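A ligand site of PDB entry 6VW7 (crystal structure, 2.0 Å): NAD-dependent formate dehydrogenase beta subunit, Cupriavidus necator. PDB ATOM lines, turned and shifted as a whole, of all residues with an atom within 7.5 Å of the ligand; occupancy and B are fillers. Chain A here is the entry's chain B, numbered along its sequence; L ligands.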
ATOM      1  N   VAL A 271     -24.821  34.213  12.816  1.00  0.00           N
ATOM      2  CA  VAL A 271     -23.610  33.435  12.560  1.00  0.00           C
ATOM      3  C   VAL A 271     -22.885  33.846  11.275  1.00  0.00           C
ATOM      4  O   VAL A 271     -21.724  33.497  11.101  1.00  0.00           O
ATOM      5  CB  VAL A 271     -23.958  31.936  12.601  1.00  0.00           C
ATOM      6  CG1 VAL A 271     -22.760  31.043  12.246  1.00  0.00           C
ATOM      7  CG2 VAL A 271     -24.384  31.592  14.008  1.00  0.00           C
ATOM      8  N   GLU A 274     -19.401  35.098  11.493  1.00  0.00           N
ATOM      9  CA  GLU A 274     -18.252  34.190  11.466  1.00  0.00           C
ATOM     10  C   GLU A 274     -17.688  34.161  10.035  1.00  0.00           C
ATOM     11  O   GLU A 274     -18.442  33.970   9.081  1.00  0.00           O
ATOM     12  CB  GLU A 274     -18.693  32.800  11.915  1.00  0.00           C
ATOM     13  CG  GLU A 274     -17.577  31.872  12.366  1.00  0.00           C
ATOM     14  CD  GLU A 274     -16.821  31.223  11.216  1.00  0.00           C
ATOM     15  OE1 GLU A 274     -17.360  31.102  10.088  1.00  0.00           O
ATOM     16  OE2 GLU A 274     -15.681  30.815  11.454  1.00  0.00           O
ATOM     17  N   ALA A 277     -18.712  31.412   7.501  1.00  0.00           N
ATOM     18  CA  ALA A 277     -20.146  31.418   7.200  1.00  0.00           C
ATOM     19  C   ALA A 277     -20.500  32.637   6.356  1.00  0.00           C
ATOM     20  O   ALA A 277     -21.363  32.559   5.472  1.00  0.00           O
ATOM     21  CB  ALA A 277     -20.981  31.408   8.490  1.00  0.00           C
ATOM     22  N   GLY A 287     -25.509  29.911   5.593  1.00  0.00           N
ATOM     23  CA  GLY A 287     -24.377  30.425   6.350  1.00  0.00           C
ATOM     24  C   GLY A 287     -23.815  29.418   7.340  1.00  0.00           C
ATOM     25  O   GLY A 287     -23.839  29.634   8.548  1.00  0.00           O
ATOM     26  N   VAL A 288     -23.304  28.294   6.831  1.00  0.00           N
ATOM     27  CA  VAL A 288     -22.779  27.225   7.677  1.00  0.00           C
ATOM     28  C   VAL A 288     -21.267  27.369   7.775  1.00  0.00           C
ATOM     29  O   VAL A 288     -20.577  27.468   6.756  1.00  0.00           O
ATOM     30  CB  VAL A 288     -23.181  25.848   7.118  1.00  0.00           C
ATOM     31  CG1 VAL A 288     -22.562  24.701   7.967  1.00  0.00           C
ATOM     32  CG2 VAL A 288     -24.706  25.726   7.057  1.00  0.00           C
ATOM     33  N   VAL A 289     -20.745  27.401   9.009  1.00  0.00           N
ATOM     34  CA  VAL A 289     -19.313  27.571   9.216  1.00  0.00           C
ATOM     35  C   VAL A 289     -18.532  26.501   8.459  1.00  0.00           C
ATOM     36  O   VAL A 289     -18.919  25.325   8.437  1.00  0.00           O
ATOM     37  CB  VAL A 289     -19.011  27.506  10.713  1.00  0.00           C
ATOM     38  CG1 VAL A 289     -17.512  27.507  10.978  1.00  0.00           C
ATOM     39  CG2 VAL A 289     -19.683  28.661  11.451  1.00  0.00           C
ATOM     40  N   ARG A 290     -17.422  26.899   7.825  1.00  0.00           N
ATOM     41  CA  ARG A 290     -16.527  25.952   7.154  1.00  0.00           C
ATOM     42  C   ARG A 290     -15.493  25.424   8.157  1.00  0.00           C
ATOM     43  O   ARG A 290     -15.073  26.135   9.073  1.00  0.00           O
ATOM     44  CB  ARG A 290     -15.772  26.617   6.000  1.00  0.00           C
ATOM     45  CG  ARG A 290     -16.611  27.088   4.826  1.00  0.00           C
ATOM     46  CD  ARG A 290     -15.757  28.015   3.926  1.00  0.00           C
ATOM     47  NE  ARG A 290     -16.463  28.514   2.749  1.00  0.00           N
ATOM     48  CZ  ARG A 290     -15.897  29.229   1.777  1.00  0.00           C
ATOM     49  NH1 ARG A 290     -14.616  29.553   1.831  1.00  0.00           N
ATOM     50  NH2 ARG A 290     -16.635  29.610   0.746  1.00  0.00           N
ATOM     51  N   CYS A 438     -28.493  31.322  21.292  1.00  0.00           N
ATOM     52  CA  CYS A 438     -27.684  30.317  20.604  1.00  0.00           C
ATOM     53  C   CYS A 438     -28.560  29.331  19.857  1.00  0.00           C
ATOM     54  O   CYS A 438     -28.250  28.945  18.723  1.00  0.00           O
ATOM     55  CB  CYS A 438     -26.798  29.581  21.620  1.00  0.00           C
ATOM     56  SG  CYS A 438     -25.663  28.386  20.848  1.00  0.00           S
ATOM     57  N   GLU A 441     -29.752  31.145  16.704  1.00  0.00           N
ATOM     58  CA  GLU A 441     -28.778  31.500  15.674  1.00  0.00           C
ATOM     59  C   GLU A 441     -27.898  30.343  15.231  1.00  0.00           C
ATOM     60  O   GLU A 441     -27.114  30.518  14.292  1.00  0.00           O
ATOM     61  CB  GLU A 441     -27.888  32.643  16.166  1.00  0.00           C
ATOM     62  CG  GLU A 441     -28.671  33.900  16.550  1.00  0.00           C
ATOM     63  CD  GLU A 441     -29.343  34.563  15.336  1.00  0.00           C
ATOM     64  OE1 GLU A 441     -29.072  34.192  14.175  1.00  0.00           O
ATOM     65  OE2 GLU A 441     -30.176  35.465  15.556  1.00  0.00           O
ATOM     66  N   SER A 442     -27.994  29.172  15.853  1.00  0.00           N
ATOM     67  CA  SER A 442     -27.088  28.083  15.509  1.00  0.00           C
ATOM     68  C   SER A 442     -27.183  27.757  14.022  1.00  0.00           C
ATOM     69  O   SER A 442     -28.271  27.576  13.479  1.00  0.00           O
ATOM     70  CB  SER A 442     -27.410  26.848  16.330  1.00  0.00           C
ATOM     71  OG  SER A 442     -26.694  25.727  15.847  1.00  0.00           O
ATOM     72  N   CYS A 443     -26.028  27.696  13.349  1.00  0.00           N
ATOM     73  CA  CYS A 443     -26.012  27.266  11.956  1.00  0.00           C
ATOM     74  C   CYS A 443     -26.348  25.784  11.818  1.00  0.00           C
ATOM     75  O   CYS A 443     -26.683  25.326  10.712  1.00  0.00           O
ATOM     76  CB  CYS A 443     -24.669  27.632  11.296  1.00  0.00           C
ATOM     77  SG  CYS A 443     -23.369  26.369  11.341  1.00  0.00           S
ATOM     78  N   GLY A 444     -26.277  25.015  12.905  1.00  0.00           N
ATOM     79  CA  GLY A 444     -26.760  23.648  12.914  1.00  0.00           C
ATOM     80  C   GLY A 444     -25.715  22.565  12.755  1.00  0.00           C
ATOM     81  O   GLY A 444     -26.050  21.384  12.835  1.00  0.00           O
ATOM     82  N   LYS A 445     -24.452  22.942  12.521  1.00  0.00           N
ATOM     83  CA  LYS A 445     -23.421  21.962  12.231  1.00  0.00           C
ATOM     84  C   LYS A 445     -23.038  21.133  13.466  1.00  0.00           C
ATOM     85  O   LYS A 445     -22.650  19.967  13.330  1.00  0.00           O
ATOM     86  CB  LYS A 445     -22.210  22.698  11.653  1.00  0.00           C
ATOM     87  CG  LYS A 445     -21.091  21.838  11.099  1.00  0.00           C
ATOM     88  CD  LYS A 445     -19.935  22.724  10.614  1.00  0.00           C
ATOM     89  CE  LYS A 445     -19.252  22.126   9.382  1.00  0.00           C
ATOM     90  NZ  LYS A 445     -18.116  22.957   8.885  1.00  0.00           N
ATOM     91  N   CYS A 446     -23.183  21.693  14.672  1.00  0.00           N
ATOM     92  CA  CYS A 446     -22.691  21.091  15.913  1.00  0.00           C
ATOM     93  C   CYS A 446     -23.861  20.782  16.832  1.00  0.00           C
ATOM     94  O   CYS A 446     -24.736  21.628  17.038  1.00  0.00           O
ATOM     95  CB  CYS A 446     -21.721  22.032  16.632  1.00  0.00           C
ATOM     96  SG  CYS A 446     -20.277  22.530  15.641  1.00  0.00           S
ATOM     97  N   THR A 447     -23.871  19.574  17.397  1.00  0.00           N
ATOM     98  CA  THR A 447     -24.995  19.163  18.241  1.00  0.00           C
ATOM     99  C   THR A 447     -25.109  19.973  19.532  1.00  0.00           C
ATOM    100  O   THR A 447     -26.223  20.412  19.865  1.00  0.00           O
ATOM    101  CB  THR A 447     -24.918  17.659  18.507  1.00  0.00           C
ATOM    102  OG1 THR A 447     -25.075  16.968  17.269  1.00  0.00           O
ATOM    103  CG2 THR A 447     -26.032  17.232  19.461  1.00  0.00           C
ATOM    104  N   PRO A 448     -24.038  20.195  20.294  1.00  0.00           N
ATOM    105  CA  PRO A 448     -24.214  20.995  21.522  1.00  0.00           C
ATOM    106  C   PRO A 448     -24.763  22.381  21.233  1.00  0.00           C
ATOM    107  O   PRO A 448     -25.612  22.885  21.965  1.00  0.00           O
ATOM    108  CB  PRO A 448     -22.794  21.041  22.112  1.00  0.00           C
ATOM    109  CG  PRO A 448     -22.100  19.857  21.523  1.00  0.00           C
ATOM    110  CD  PRO A 448     -22.640  19.764  20.130  1.00  0.00           C
ATOM    111  N   CYS A 449     -24.327  22.994  20.126  1.00  0.00           N
ATOM    112  CA  CYS A 449     -24.829  24.325  19.783  1.00  0.00           C
ATOM    113  C   CYS A 449     -26.273  24.280  19.292  1.00  0.00           C
ATOM    114  O   CYS A 449     -27.092  25.126  19.664  1.00  0.00           O
ATOM    115  CB  CYS A 449     -23.930  24.953  18.739  1.00  0.00           C
ATOM    116  SG  CYS A 449     -24.544  26.569  18.184  1.00  0.00           S
ATOM    117  N   ARG A 450     -26.609  23.308  18.446  1.00  0.00           N
ATOM    118  CA  ARG A 450     -27.918  23.284  17.804  1.00  0.00           C
ATOM    119  C   ARG A 450     -29.018  22.794  18.746  1.00  0.00           C
ATOM    120  O   ARG A 450     -30.116  23.353  18.754  1.00  0.00           O
ATOM    121  CB  ARG A 450     -27.871  22.415  16.552  1.00  0.00           C
ATOM    122  CG  ARG A 450     -29.197  22.313  15.810  1.00  0.00           C
ATOM    123  CD  ARG A 450     -29.039  21.395  14.609  1.00  0.00           C
ATOM    124  NE  ARG A 450     -28.106  20.319  14.894  1.00  0.00           N
ATOM    125  CZ  ARG A 450     -28.432  19.063  15.152  1.00  0.00           C
ATOM    126  NH1 ARG A 450     -27.479  18.177  15.397  1.00  0.00           N
ATOM    127  NH2 ARG A 450     -29.707  18.698  15.158  1.00  0.00           N
ATOM    128  N   MET A 483     -20.407  22.449  25.388  1.00  0.00           N
ATOM    129  CA  MET A 483     -20.319  23.466  24.356  1.00  0.00           C
ATOM    130  C   MET A 483     -18.902  24.008  24.240  1.00  0.00           C
ATOM    131  O   MET A 483     -18.435  24.281  23.133  1.00  0.00           O
ATOM    132  CB  MET A 483     -21.309  24.603  24.638  1.00  0.00           C
ATOM    133  CG  MET A 483     -22.763  24.144  24.594  1.00  0.00           C
ATOM    134  SD  MET A 483     -23.886  25.453  25.119  1.00  0.00           S
ATOM    135  CE  MET A 483     -24.241  26.220  23.540  1.00  0.00           C
ATOM    136  N   GLY A 486     -17.136  21.119  22.286  1.00  0.00           N
ATOM    137  CA  GLY A 486     -17.736  20.468  21.138  1.00  0.00           C
ATOM    138  C   GLY A 486     -18.353  21.423  20.144  1.00  0.00           C
ATOM    139  O   GLY A 486     -19.295  21.052  19.439  1.00  0.00           O
ATOM    140  N   SER A 487     -17.846  22.646  20.082  1.00  0.00           N
ATOM    141  CA  SER A 487     -18.365  23.671  19.178  1.00  0.00           C
ATOM    142  C   SER A 487     -17.296  24.007  18.154  1.00  0.00           C
ATOM    143  O   SER A 487     -16.128  24.201  18.516  1.00  0.00           O
ATOM    144  CB  SER A 487     -18.761  24.934  19.941  1.00  0.00           C
ATOM    145  OG  SER A 487     -19.856  24.701  20.814  1.00  0.00           O
ATOM    146  N   LEU A 488     -17.676  24.056  16.877  1.00  0.00           N
ATOM    147  CA  LEU A 488     -16.715  24.346  15.817  1.00  0.00           C
ATOM    148  C   LEU A 488     -16.472  25.838  15.613  1.00  0.00           C
ATOM    149  O   LEU A 488     -15.517  26.208  14.910  1.00  0.00           O
ATOM    150  CB  LEU A 488     -17.168  23.689  14.505  1.00  0.00           C
ATOM    151  CG  LEU A 488     -17.042  22.149  14.534  1.00  0.00           C
ATOM    152  CD1 LEU A 488     -17.741  21.457  13.359  1.00  0.00           C
ATOM    153  CD2 LEU A 488     -15.581  21.689  14.647  1.00  0.00           C
ATOM    154  N   CYS A 489     -17.294  26.719  16.197  1.00  0.00           N
ATOM    155  CA  CYS A 489     -16.998  28.147  16.179  1.00  0.00           C
ATOM    156  C   CYS A 489     -17.485  28.770  17.491  1.00  0.00           C
ATOM    157  O   CYS A 489     -18.049  28.082  18.355  1.00  0.00           O
ATOM    158  CB  CYS A 489     -17.620  28.838  14.949  1.00  0.00           C
ATOM    159  SG  CYS A 489     -19.282  29.348  15.225  1.00  0.00           S
ATOM    160  N   ALA A 490     -17.260  30.070  17.627  1.00  0.00           N
ATOM    161  CA  ALA A 490     -17.483  30.741  18.910  1.00  0.00           C
ATOM    162  C   ALA A 490     -18.953  30.923  19.262  1.00  0.00           C
ATOM    163  O   ALA A 490     -19.253  31.236  20.431  1.00  0.00           O
ATOM    164  CB  ALA A 490     -16.786  32.101  18.924  1.00  0.00           C
ATOM    165  N   MET A 491     -19.884  30.761  18.311  1.00  0.00           N
ATOM    166  CA  MET A 491     -21.299  30.809  18.670  1.00  0.00           C
ATOM    167  C   MET A 491     -21.602  29.787  19.767  1.00  0.00           C
ATOM    168  O   MET A 491     -22.003  30.139  20.884  1.00  0.00           O
ATOM    169  CB  MET A 491     -22.173  30.546  17.436  1.00  0.00           C
ATOM    170  CG  MET A 491     -23.654  30.439  17.760  1.00  0.00           C
ATOM    171  SD  MET A 491     -24.432  32.082  17.929  1.00  0.00           S
ATOM    172  CE  MET A 491     -24.500  32.303  19.699  1.00  0.00           C
ATOM    173  N   GLY A 492     -21.385  28.502  19.480  1.00  0.00           N
ATOM    174  CA  GLY A 492     -21.537  27.504  20.512  1.00  0.00           C
ATOM    175  C   GLY A 492     -20.419  27.575  21.548  1.00  0.00           C
ATOM    176  O   GLY A 492     -20.652  27.354  22.736  1.00  0.00           O
ATOM    177  N   GLY A 493     -19.215  27.897  21.104  1.00  0.00           N
ATOM    178  CA  GLY A 493     -18.062  27.781  21.975  1.00  0.00           C
ATOM    179  C   GLY A 493     -18.004  28.840  23.059  1.00  0.00           C
ATOM    180  O   GLY A 493     -17.415  28.608  24.120  1.00  0.00           O
ATOM    181  N   MET A 494     -18.616  30.005  22.815  1.00  0.00           N
ATOM    182  CA  MET A 494     -18.583  31.097  23.779  1.00  0.00           C
ATOM    183  C   MET A 494     -19.939  31.396  24.399  1.00  0.00           C
ATOM    184  O   MET A 494     -20.044  32.309  25.231  1.00  0.00           O
ATOM    185  CB  MET A 494     -17.992  32.352  23.141  1.00  0.00           C
ATOM    186  CG  MET A 494     -16.480  32.306  22.934  1.00  0.00           C
ATOM    187  SD  MET A 494     -15.851  33.704  21.960  1.00  0.00           S
ATOM    188  CE  MET A 494     -16.041  35.089  23.085  1.00  0.00           C
HETATM  189 FE1  LIG L   1     -20.669  27.440  15.212  1.00  0.00          FE
HETATM  190 FE2  LIG L   1     -21.221  24.770  15.372  1.00  0.00          FE
HETATM  191 FE3  LIG L   1     -22.611  26.314  13.639  1.00  0.00          FE
HETATM  192 FE4  LIG L   1     -22.908  26.578  16.345  1.00  0.00          FE
HETATM  193  S1  LIG L   1     -23.488  24.791  15.037  1.00  0.00           S
HETATM  194  S2  LIG L   1     -22.789  28.269  14.811  1.00  0.00           S
HETATM  195  S3  LIG L   1     -20.783  26.209  17.104  1.00  0.00           S
HETATM  196  S4  LIG L   1     -20.375  25.832  13.598  1.00  0.00           S
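N of Cys 446 sits close to S1 of the ligand.
The backbone NH (N) of Cys 443 sits close to a sulfur (S2) of the ligand, at 3.6 Å.
An iron atom (FE1) of the ligand is bound by the side-chain sulfur of Cys 489 (2.4 Å).
The backbone NH of Leu 488 sits close to a sulfur (S3) of the ligand.
The side-chain hydroxyl (OG) of Ser 442 sits close to a sulfur (S1) of the ligand (3.4 Å).
The side-chain sulfur (SG) of Cys 443 is bound to an iron atom (FE3) of the ligand (2.4 Å).
The side-chain sulfur of Cys 449 binds an iron atom (FE4) of the ligand.
The backbone NH (N) of Cys 489 lies close to a sulfur (S3) of the ligand (3.6 Å).
The backbone NH of Lys 445 lies close to a sulfur (S1) of the ligand.
An iron atom (FE2) of the ligand is bound by the side-chain sulfur (SG) of Cys 446 (2.4 Å).
S3 of the ligand lies close to N of Gly 492 (3.4 Å).
The backbone NH of Gly 444 lies close to a sulfur (S1) of the ligand (3.5 Å).
O of Gly 492 sits close to OG of Ser 487.
The backbone carbonyl oxygen of Cys 449 lies within hydrogen-bond range of the side-chain sulfur of Cys 438 (3.8 Å).
The backbone carbonyl oxygen (O) of Gly 444 sits at hydrogen-bond distance from the guanidinium group (NE) of Arg 450, 3.1 Å away.
The backbone NH (N) of Val 289 sits close to the side-chain sulfur (SG) of Cys 443, at 3.7 Å.
OG of Ser 487 sits at hydrogen-bond distance from O of Met 483, 2.8 Å away.
The backbone NH of Lys 445 lies close to the side-chain sulfur of Cys 443.
The backbone NH (N) of Gly 444 is in hydrogen-bond range of the side-chain hydroxyl (OG) of Ser 442, at 3.1 Å.
The side-chain sulfur (SG) of Cys 489 sits close to the backbone NH (N) of Met 491, 3.4 Å away.
Val 271 touches the ligand (CG2 to S2, 3.8 Å).
Val 289 touches the ligand.
Ser 487 touches the ligand.
Met 491 touches the ligand.
Hydrophobic or aromatic side chains within 4 Å of the ligand: Val 271, Val 289, Leu 488 and Met 491.
Of the 28 residues printed, 13 come within 4 Å of the ligand.
The nearest printed residue that does not touch the ligand is Gly 493 (4.6 Å).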
